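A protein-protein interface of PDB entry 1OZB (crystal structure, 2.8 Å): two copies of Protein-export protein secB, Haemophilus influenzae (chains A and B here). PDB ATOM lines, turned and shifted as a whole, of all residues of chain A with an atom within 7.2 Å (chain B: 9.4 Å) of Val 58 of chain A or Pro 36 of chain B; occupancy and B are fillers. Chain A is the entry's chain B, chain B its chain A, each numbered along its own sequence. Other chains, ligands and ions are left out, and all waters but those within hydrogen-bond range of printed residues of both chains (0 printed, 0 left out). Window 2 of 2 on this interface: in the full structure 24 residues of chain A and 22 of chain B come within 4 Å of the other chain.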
ATOM      1  N   ARG A  22      26.631  20.250   8.835  1.00  0.00           N
ATOM      2  CA  ARG A  22      27.668  20.552   7.865  1.00  0.00           C
ATOM      3  C   ARG A  22      27.410  21.875   7.149  1.00  0.00           C
ATOM      4  O   ARG A  22      26.269  22.243   6.892  1.00  0.00           O
ATOM      5  CB  ARG A  22      27.750  19.428   6.832  1.00  0.00           C
ATOM      6  CG  ARG A  22      29.009  19.464   5.969  1.00  0.00           C
ATOM      7  CD  ARG A  22      28.805  18.678   4.674  1.00  0.00           C
ATOM      8  NE  ARG A  22      28.519  17.269   4.919  1.00  0.00           N
ATOM      9  CZ  ARG A  22      29.448  16.337   5.073  1.00  0.00           C
ATOM     10  NH1 ARG A  22      30.735  16.655   5.001  1.00  0.00           N
ATOM     11  NH2 ARG A  22      29.088  15.086   5.316  1.00  0.00           N
ATOM     12  N   TYR A  24      28.663  23.829   3.688  1.00  0.00           N
ATOM     13  CA  TYR A  24      29.409  23.631   2.451  1.00  0.00           C
ATOM     14  C   TYR A  24      28.887  24.498   1.331  1.00  0.00           C
ATOM     15  O   TYR A  24      27.795  25.047   1.423  1.00  0.00           O
ATOM     16  CB  TYR A  24      29.334  22.164   2.029  1.00  0.00           C
ATOM     17  CG  TYR A  24      27.918  21.641   1.925  1.00  0.00           C
ATOM     18  CD1 TYR A  24      27.200  21.731   0.724  1.00  0.00           C
ATOM     19  CD2 TYR A  24      27.269  21.106   3.043  1.00  0.00           C
ATOM     20  CE1 TYR A  24      25.874  21.303   0.644  1.00  0.00           C
ATOM     21  CE2 TYR A  24      25.944  20.677   2.982  1.00  0.00           C
ATOM     22  CZ  TYR A  24      25.252  20.779   1.781  1.00  0.00           C
ATOM     23  OH  TYR A  24      23.938  20.365   1.721  1.00  0.00           O
ATOM     24  N   LYS A  26      27.661  24.705  -2.544  1.00  0.00           N
ATOM     25  CA  LYS A  26      27.168  23.861  -3.627  1.00  0.00           C
ATOM     26  C   LYS A  26      27.593  24.400  -4.986  1.00  0.00           C
ATOM     27  O   LYS A  26      27.821  23.625  -5.917  1.00  0.00           O
ATOM     28  CB  LYS A  26      25.645  23.750  -3.567  1.00  0.00           C
ATOM     29  CG  LYS A  26      25.115  23.071  -2.304  1.00  0.00           C
ATOM     30  CD  LYS A  26      23.573  23.086  -2.219  1.00  0.00           C
ATOM     31  CE  LYS A  26      22.900  22.177  -3.244  1.00  0.00           C
ATOM     32  NZ  LYS A  26      23.347  20.775  -3.073  1.00  0.00           N
ATOM     33  N   THR A  56      15.215  22.139   1.838  1.00  0.00           N
ATOM     34  CA  THR A  56      14.880  20.815   1.359  1.00  0.00           C
ATOM     35  C   THR A  56      15.176  19.824   2.461  1.00  0.00           C
ATOM     36  O   THR A  56      16.262  19.836   3.039  1.00  0.00           O
ATOM     37  CB  THR A  56      15.696  20.431   0.113  1.00  0.00           C
ATOM     38  OG1 THR A  56      15.124  21.048  -1.043  1.00  0.00           O
ATOM     39  CG2 THR A  56      15.700  18.921  -0.076  1.00  0.00           C
ATOM     40  N   GLN A  57      14.200  18.979   2.779  1.00  0.00           N
ATOM     41  CA  GLN A  57      14.435  17.990   3.811  1.00  0.00           C
ATOM     42  C   GLN A  57      15.266  16.899   3.161  1.00  0.00           C
ATOM     43  O   GLN A  57      14.939  16.395   2.087  1.00  0.00           O
ATOM     44  CB  GLN A  57      13.134  17.428   4.362  1.00  0.00           C
ATOM     45  CG  GLN A  57      13.372  16.480   5.524  1.00  0.00           C
ATOM     46  CD  GLN A  57      12.118  16.232   6.336  1.00  0.00           C
ATOM     47  OE1 GLN A  57      11.064  16.800   6.049  1.00  0.00           O
ATOM     48  NE2 GLN A  57      12.224  15.390   7.363  1.00  0.00           N
ATOM     49  N   VAL A  58      16.363  16.556   3.813  1.00  0.00           N
ATOM     50  CA  VAL A  58      17.269  15.562   3.277  1.00  0.00           C
ATOM     51  C   VAL A  58      17.345  14.323   4.167  1.00  0.00           C
ATOM     52  O   VAL A  58      18.145  13.417   3.922  1.00  0.00           O
ATOM     53  CB  VAL A  58      18.676  16.170   3.117  1.00  0.00           C
ATOM     54  CG1 VAL A  58      19.227  16.535   4.480  1.00  0.00           C
ATOM     55  CG2 VAL A  58      19.599  15.200   2.393  1.00  0.00           C
ATOM     56  N   GLY A  59      16.504  14.284   5.196  1.00  0.00           N
ATOM     57  CA  GLY A  59      16.496  13.152   6.107  1.00  0.00           C
ATOM     58  C   GLY A  59      15.510  13.380   7.233  1.00  0.00           C
ATOM     59  O   GLY A  59      14.737  14.331   7.198  1.00  0.00           O
ATOM     60  N   ASP A  60      15.517  12.501   8.227  1.00  0.00           N
ATOM     61  CA  ASP A  60      14.620  12.662   9.363  1.00  0.00           C
ATOM     62  C   ASP A  60      15.174  13.789  10.214  1.00  0.00           C
ATOM     63  O   ASP A  60      16.265  13.659  10.773  1.00  0.00           O
ATOM     64  CB  ASP A  60      14.580  11.389  10.202  1.00  0.00           C
ATOM     65  CG  ASP A  60      13.894  10.251   9.497  1.00  0.00           C
ATOM     66  OD1 ASP A  60      12.674  10.363   9.257  1.00  0.00           O
ATOM     67  OD2 ASP A  60      14.574   9.251   9.183  1.00  0.00           O
ATOM     68  N   ASP A  61      14.441  14.893  10.315  1.00  0.00           N
ATOM     69  CA  ASP A  61      14.909  16.023  11.118  1.00  0.00           C
ATOM     70  C   ASP A  61      16.146  16.668  10.504  1.00  0.00           C
ATOM     71  O   ASP A  61      16.812  17.457  11.161  1.00  0.00           O
ATOM     72  CB  ASP A  61      15.276  15.566  12.529  1.00  0.00           C
ATOM     73  CG  ASP A  61      14.111  14.974  13.271  1.00  0.00           C
ATOM     74  OD1 ASP A  61      14.349  14.206  14.233  1.00  0.00           O
ATOM     75  OD2 ASP A  61      12.961  15.286  12.899  1.00  0.00           O
ATOM     76  N   LEU A  62      16.464  16.315   9.262  1.00  0.00           N
ATOM     77  CA  LEU A  62      17.628  16.869   8.581  1.00  0.00           C
ATOM     78  C   LEU A  62      17.187  17.701   7.405  1.00  0.00           C
ATOM     79  O   LEU A  62      16.521  17.200   6.500  1.00  0.00           O
ATOM     80  CB  LEU A  62      18.563  15.763   8.095  1.00  0.00           C
ATOM     81  CG  LEU A  62      19.480  15.186   9.167  1.00  0.00           C
ATOM     82  CD1 LEU A  62      20.491  14.249   8.534  1.00  0.00           C
ATOM     83  CD2 LEU A  62      20.192  16.334   9.874  1.00  0.00           C
ATOM     84  N   TYR A  63      17.560  18.975   7.420  1.00  0.00           N
ATOM     85  CA  TYR A  63      17.180  19.875   6.349  1.00  0.00           C
ATOM     86  C   TYR A  63      18.397  20.584   5.802  1.00  0.00           C
ATOM     87  O   TYR A  63      19.302  20.949   6.552  1.00  0.00           O
ATOM     88  CB  TYR A  63      16.183  20.913   6.867  1.00  0.00           C
ATOM     89  CG  TYR A  63      15.024  20.330   7.638  1.00  0.00           C
ATOM     90  CD1 TYR A  63      15.240  19.604   8.811  1.00  0.00           C
ATOM     91  CD2 TYR A  63      13.709  20.489   7.192  1.00  0.00           C
ATOM     92  CE1 TYR A  63      14.182  19.046   9.519  1.00  0.00           C
ATOM     93  CE2 TYR A  63      12.636  19.935   7.899  1.00  0.00           C
ATOM     94  CZ  TYR A  63      12.884  19.213   9.059  1.00  0.00           C
ATOM     95  OH  TYR A  63      11.850  18.634   9.754  1.00  0.00           O
ATOM     96  N   GLU A  64      18.421  20.766   4.488  1.00  0.00           N
ATOM     97  CA  GLU A  64      19.515  21.470   3.849  1.00  0.00           C
ATOM     98  C   GLU A  64      18.991  22.856   3.537  1.00  0.00           C
ATOM     99  O   GLU A  64      18.059  23.000   2.741  1.00  0.00           O
ATOM    100  CB  GLU A  64      19.926  20.805   2.538  1.00  0.00           C
ATOM    101  CG  GLU A  64      20.964  21.613   1.748  1.00  0.00           C
ATOM    102  CD  GLU A  64      20.930  21.309   0.252  1.00  0.00           C
ATOM    103  OE1 GLU A  64      19.828  21.365  -0.334  1.00  0.00           O
ATOM    104  OE2 GLU A  64      21.991  21.024  -0.346  1.00  0.00           O
ATOM    105  N   GLY A  91      23.933  24.556   4.138  1.00  0.00           N
ATOM    106  CA  GLY A  91      24.216  23.913   5.404  1.00  0.00           C
ATOM    107  C   GLY A  91      23.173  22.851   5.691  1.00  0.00           C
ATOM    108  O   GLY A  91      22.025  23.001   5.288  1.00  0.00           O
ATOM    109  N   VAL A  92      23.575  21.763   6.344  1.00  0.00           N
ATOM    110  CA  VAL A  92      22.639  20.704   6.716  1.00  0.00           C
ATOM    111  C   VAL A  92      22.398  20.875   8.208  1.00  0.00           C
ATOM    112  O   VAL A  92      23.342  20.850   9.005  1.00  0.00           O
ATOM    113  CB  VAL A  92      23.214  19.279   6.487  1.00  0.00           C
ATOM    114  CG1 VAL A  92      22.334  18.252   7.173  1.00  0.00           C
ATOM    115  CG2 VAL A  92      23.268  18.960   5.011  1.00  0.00           C
ATOM    116  N   PHE A  93      21.141  21.060   8.597  1.00  0.00           N
ATOM    117  CA  PHE A  93      20.832  21.243  10.009  1.00  0.00           C
ATOM    118  C   PHE A  93      19.881  20.188  10.516  1.00  0.00           C
ATOM    119  O   PHE A  93      19.074  19.652   9.762  1.00  0.00           O
ATOM    120  CB  PHE A  93      20.185  22.608  10.266  1.00  0.00           C
ATOM    121  CG  PHE A  93      20.958  23.764   9.725  1.00  0.00           C
ATOM    122  CD1 PHE A  93      20.982  24.024   8.358  1.00  0.00           C
ATOM    123  CD2 PHE A  93      21.664  24.598  10.582  1.00  0.00           C
ATOM    124  CE1 PHE A  93      21.697  25.095   7.849  1.00  0.00           C
ATOM    125  CE2 PHE A  93      22.385  25.676  10.084  1.00  0.00           C
ATOM    126  CZ  PHE A  93      22.401  25.925   8.707  1.00  0.00           C
ATOM    127  N   ALA B  32      29.432  21.572  -6.796  1.00  0.00           N
ATOM    128  CA  ALA B  32      29.312  20.280  -6.135  1.00  0.00           C
ATOM    129  C   ALA B  32      27.816  19.993  -6.187  1.00  0.00           C
ATOM    130  O   ALA B  32      27.089  20.178  -5.201  1.00  0.00           O
ATOM    131  CB  ALA B  32      29.800  20.358  -4.699  1.00  0.00           C
ATOM    132  N   PRO B  33      27.341  19.533  -7.353  1.00  0.00           N
ATOM    133  CA  PRO B  33      25.937  19.211  -7.612  1.00  0.00           C
ATOM    134  C   PRO B  33      25.287  18.140  -6.768  1.00  0.00           C
ATOM    135  O   PRO B  33      24.110  18.266  -6.445  1.00  0.00           O
ATOM    136  CB  PRO B  33      25.928  18.867  -9.094  1.00  0.00           C
ATOM    137  CG  PRO B  33      27.283  18.277  -9.303  1.00  0.00           C
ATOM    138  CD  PRO B  33      28.175  19.211  -8.525  1.00  0.00           C
ATOM    139  N   ASN B  34      26.042  17.118  -6.378  1.00  0.00           N
ATOM    140  CA  ASN B  34      25.473  16.027  -5.608  1.00  0.00           C
ATOM    141  C   ASN B  34      25.624  16.088  -4.087  1.00  0.00           C
ATOM    142  O   ASN B  34      25.865  15.071  -3.442  1.00  0.00           O
ATOM    143  CB  ASN B  34      26.029  14.707  -6.151  1.00  0.00           C
ATOM    144  CG  ASN B  34      25.953  14.631  -7.669  1.00  0.00           C
ATOM    145  OD1 ASN B  34      24.899  14.872  -8.255  1.00  0.00           O
ATOM    146  ND2 ASN B  34      27.082  14.295  -8.313  1.00  0.00           N
ATOM    147  N   LEU B  35      25.478  17.275  -3.509  1.00  0.00           N
ATOM    148  CA  LEU B  35      25.560  17.398  -2.060  1.00  0.00           C
ATOM    149  C   LEU B  35      24.151  17.509  -1.479  1.00  0.00           C
ATOM    150  O   LEU B  35      23.233  18.018  -2.131  1.00  0.00           O
ATOM    151  CB  LEU B  35      26.420  18.597  -1.655  1.00  0.00           C
ATOM    152  CG  LEU B  35      27.909  18.251  -1.678  1.00  0.00           C
ATOM    153  CD1 LEU B  35      28.305  17.896  -3.099  1.00  0.00           C
ATOM    154  CD2 LEU B  35      28.741  19.407  -1.177  1.00  0.00           C
ATOM    155  N   PRO B  36      23.967  17.040  -0.238  1.00  0.00           N
ATOM    156  CA  PRO B  36      24.972  16.435   0.633  1.00  0.00           C
ATOM    157  C   PRO B  36      25.107  14.912   0.568  1.00  0.00           C
ATOM    158  O   PRO B  36      26.008  14.351   1.197  1.00  0.00           O
ATOM    159  CB  PRO B  36      24.508  16.871   1.994  1.00  0.00           C
ATOM    160  CG  PRO B  36      23.033  16.619   1.856  1.00  0.00           C
ATOM    161  CD  PRO B  36      22.701  17.208   0.491  1.00  0.00           C
ATOM    162  N   HIS B  37      24.225  14.244  -0.174  1.00  0.00           N
ATOM    163  CA  HIS B  37      24.262  12.785  -0.269  1.00  0.00           C
ATOM    164  C   HIS B  37      25.559  12.156  -0.768  1.00  0.00           C
ATOM    165  O   HIS B  37      25.892  11.037  -0.377  1.00  0.00           O
ATOM    166  CB  HIS B  37      23.102  12.281  -1.120  1.00  0.00           C
ATOM    167  CG  HIS B  37      22.806  13.135  -2.310  1.00  0.00           C
ATOM    168  ND1 HIS B  37      22.207  14.372  -2.206  1.00  0.00           N
ATOM    169  CD2 HIS B  37      23.002  12.922  -3.633  1.00  0.00           C
ATOM    170  CE1 HIS B  37      22.044  14.882  -3.415  1.00  0.00           C
ATOM    171  NE2 HIS B  37      22.517  14.022  -4.299  1.00  0.00           N
ATOM    172  N   ILE B  38      26.301  12.858  -1.616  1.00  0.00           N
ATOM    173  CA  ILE B  38      27.547  12.300  -2.137  1.00  0.00           C
ATOM    174  C   ILE B  38      28.500  11.943  -1.003  1.00  0.00           C
ATOM    175  O   ILE B  38      29.400  11.124  -1.177  1.00  0.00           O
ATOM    176  CB  ILE B  38      28.284  13.289  -3.093  1.00  0.00           C
ATOM    177  CG1 ILE B  38      29.335  12.541  -3.910  1.00  0.00           C
ATOM    178  CG2 ILE B  38      29.007  14.374  -2.292  1.00  0.00           C
ATOM    179  CD1 ILE B  38      28.745  11.547  -4.842  1.00  0.00           C
ATOM    180  N   PHE B  39      28.313  12.556   0.159  1.00  0.00           N
ATOM    181  CA  PHE B  39      29.203  12.269   1.268  1.00  0.00           C
ATOM    182  C   PHE B  39      28.912  10.943   1.927  1.00  0.00           C
ATOM    183  O   PHE B  39      29.600  10.541   2.861  1.00  0.00           O
ATOM    184  CB  PHE B  39      29.173  13.402   2.282  1.00  0.00           C
ATOM    185  CG  PHE B  39      29.978  14.578   1.852  1.00  0.00           C
ATOM    186  CD1 PHE B  39      29.445  15.862   1.895  1.00  0.00           C
ATOM    187  CD2 PHE B  39      31.267  14.390   1.345  1.00  0.00           C
ATOM    188  CE1 PHE B  39      30.182  16.948   1.433  1.00  0.00           C
ATOM    189  CE2 PHE B  39      32.014  15.467   0.882  1.00  0.00           C
ATOM    190  CZ  PHE B  39      31.469  16.752   0.924  1.00  0.00           C
ATOM    191  N   GLN B  40      27.900  10.257   1.410  1.00  0.00           N
ATOM    192  CA  GLN B  40      27.492   8.951   1.912  1.00  0.00           C
ATOM    193  C   GLN B  40      28.186   7.838   1.152  1.00  0.00           C
ATOM    194  O   GLN B  40      28.175   6.686   1.575  1.00  0.00           O
ATOM    195  CB  GLN B  40      25.988   8.740   1.735  1.00  0.00           C
ATOM    196  CG  GLN B  40      25.098   9.503   2.688  1.00  0.00           C
ATOM    197  CD  GLN B  40      23.634   9.429   2.282  1.00  0.00           C
ATOM    198  OE1 GLN B  40      22.768  10.004   2.941  1.00  0.00           O
ATOM    199  NE2 GLN B  40      23.354   8.725   1.189  1.00  0.00           N
ATOM    200  N   GLN B  41      28.754   8.178   0.005  1.00  0.00           N
ATOM    201  CA  GLN B  41      29.444   7.205  -0.816  1.00  0.00           C
ATOM    202  C   GLN B  41      30.885   7.025  -0.349  1.00  0.00           C
ATOM    203  O   GLN B  41      31.413   7.859   0.394  1.00  0.00           O
ATOM    204  CB  GLN B  41      29.411   7.668  -2.263  1.00  0.00           C
ATOM    205  CG  GLN B  41      28.018   7.757  -2.859  1.00  0.00           C
ATOM    206  CD  GLN B  41      28.039   8.089  -4.348  1.00  0.00           C
ATOM    207  OE1 GLN B  41      28.948   7.670  -5.088  1.00  0.00           O
ATOM    208  NE2 GLN B  41      27.033   8.832  -4.801  1.00  0.00           N
ATOM    209  N   TRP B  43      34.633   7.368  -0.405  1.00  0.00           N
ATOM    210  CA  TRP B  43      35.498   8.312  -1.067  1.00  0.00           C
ATOM    211  C   TRP B  43      36.631   7.648  -1.872  1.00  0.00           C
ATOM    212  O   TRP B  43      37.763   7.532  -1.413  1.00  0.00           O
ATOM    213  CB  TRP B  43      36.060   9.314  -0.059  1.00  0.00           C
ATOM    214  CG  TRP B  43      36.529  10.528  -0.761  1.00  0.00           C
ATOM    215  CD1 TRP B  43      37.807  10.821  -1.127  1.00  0.00           C
ATOM    216  CD2 TRP B  43      35.700  11.523  -1.358  1.00  0.00           C
ATOM    217  NE1 TRP B  43      37.825  11.935  -1.933  1.00  0.00           N
ATOM    218  CE2 TRP B  43      36.542  12.385  -2.091  1.00  0.00           C
ATOM    219  CE3 TRP B  43      34.324  11.766  -1.349  1.00  0.00           C
ATOM    220  CZ2 TRP B  43      36.058  13.471  -2.812  1.00  0.00           C
ATOM    221  CZ3 TRP B  43      33.836  12.856  -2.072  1.00  0.00           C
ATOM    222  CH2 TRP B  43      34.706  13.690  -2.793  1.00  0.00           C
ATOM    223  N   ALA B  82      31.827  14.547  -7.731  1.00  0.00           N
ATOM    224  CA  ALA B  82      31.972  15.081  -6.379  1.00  0.00           C
ATOM    225  C   ALA B  82      32.006  16.619  -6.520  1.00  0.00           C
ATOM    226  O   ALA B  82      31.227  17.338  -5.888  1.00  0.00           O
ATOM    227  CB  ALA B  82      33.261  14.562  -5.753  1.00  0.00           C
ATOM    228  N   GLY B 130      33.872  23.020   0.104  1.00  0.00           N
ATOM    229  CA  GLY B 130      32.854  22.025  -0.163  1.00  0.00           C
ATOM    230  C   GLY B 130      33.000  20.884   0.827  1.00  0.00           C
ATOM    231  O   GLY B 130      32.270  19.899   0.761  1.00  0.00           O
ATOM    232  N   THR B 131      33.940  21.041   1.761  1.00  0.00           N
ATOM    233  CA  THR B 131      34.264  20.048   2.790  1.00  0.00           C
ATOM    234  C   THR B 131      34.744  18.731   2.209  1.00  0.00           C
ATOM    235  O   THR B 131      34.490  17.686   2.773  1.00  0.00           O
ATOM    236  CB  THR B 131      33.080  19.730   3.800  1.00  0.00           C
ATOM    237  OG1 THR B 131      31.960  19.167   3.108  1.00  0.00           O
ATOM    238  CG2 THR B 131      32.654  20.980   4.546  1.00  0.00           C
ATOM    239  N   PHE B 132      35.440  18.780   1.079  1.00  0.00           N
ATOM    240  CA  PHE B 132      35.986  17.562   0.473  1.00  0.00           C
ATOM    241  C   PHE B 132      37.421  17.411   0.966  1.00  0.00           C
ATOM    242  O   PHE B 132      38.056  18.381   1.382  1.00  0.00           O
ATOM    243  CB  PHE B 132      36.004  17.642  -1.065  1.00  0.00           C
ATOM    244  CG  PHE B 132      34.644  17.783  -1.689  1.00  0.00           C
ATOM    245  CD1 PHE B 132      34.233  18.997  -2.229  1.00  0.00           C
ATOM    246  CD2 PHE B 132      33.764  16.707  -1.727  1.00  0.00           C
ATOM    247  CE1 PHE B 132      32.970  19.133  -2.796  1.00  0.00           C
ATOM    248  CE2 PHE B 132      32.497  16.835  -2.291  1.00  0.00           C
ATOM    249  CZ  PHE B 132      32.100  18.052  -2.826  1.00  0.00           C
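OG1 of Thr 131 of chain B sits at hydrogen-bond distance from NH1 of Arg 22 of chain A (3.4 Å). O of Leu 35 of chain B is in hydrogen-bond range of NZ of Lys 26 of chain A (2.9 Å). The backbone NH (N) of Ala 32 of chain B is in hydrogen-bond range of the backbone carbonyl oxygen (O) of Lys 26 of chain A (2.8 Å).
The side-chain carboxylate (OE2) of Glu 64 of chain A sits at hydrogen-bond distance from the side-chain hydroxyl (OH) of Tyr 24 of chain A, 2.9 Å away. NZ of Lys 26 of chain A is in salt-bridge range of OE2 of Glu 64 of chain A (3.1 Å). The backbone carbonyl oxygen of Thr 56 of chain A sits at hydrogen-bond distance from the backbone NH of Glu 64 of chain A, at 2.8 Å. N of Val 92 of chain A is in hydrogen-bond range of O of Arg 22 of chain A.
Among the printed residues, pairs that only touch across the chains: Arg 22 of chain A with Phe 39 of chain B, Tyr 24 of chain A with Leu 35 of chain B, Tyr 24 of chain A with Pro 36 of chain B, Tyr 24 of chain A with Gly 130 of chain B, Val 58 of chain A with Pro 36 of chain B, Glu 64 of chain A with Leu 35 of chain B, Glu 64 of chain A with Pro 36 of chain B and Val 92 of chain A with Pro 36 of chain B.
Printed residues of chain B within 4 Å of Lys 26 of chain A: Ala 32 (2.8 Å) and Leu 35 (2.9 Å). Val 58 of chain A touches one residue of chain B. No residue of chain B comes within 4 Å of Gly 59 of chain A. Of the printed residues of chain A, Ala 32 of chain B touches Lys 26. Printed residues of chain A within 4 Å of Leu 35 of chain B: Tyr 24, Lys 26 and Glu 64. Of chain A, only Tyr 24, Val 58, Glu 64 and Val 92 come within 4 Å of Pro 36 of chain B. Of the printed residues of chain A, Phe 39 of chain B touches Arg 22 (3.2 Å). Phe 132 of chain B touches none of the printed residues of chain A. The nearest residue of chain B that does not touch Val 58 of chain A is His 37 of chain B (5.4 Å). The nearest residue of chain A that does not touch Pro 36 of chain B is Lys 26 of chain A (4.7 Å).
Hydrophobic or aromatic side chains of chain A that line the printed part of chain B: Tyr 24, Val 58 and Val 92. Of the 15 printed residues of chain B, 6 touch a printed residue of chain A. Printed residues of chain B that touch a printed residue of chain A: Ala 32, Leu 35, Pro 36, Phe 39, Gly 130 and Thr 131. Hydrophobic or aromatic side chains of chain B within 4 Å of the printed part of chain A: Leu 35, Pro 36 and Phe 39.
No position is printed for both chains. Of the 11 pairs that touch across the chains among the printed residues, none has its exchanged pair printed and touching as well.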
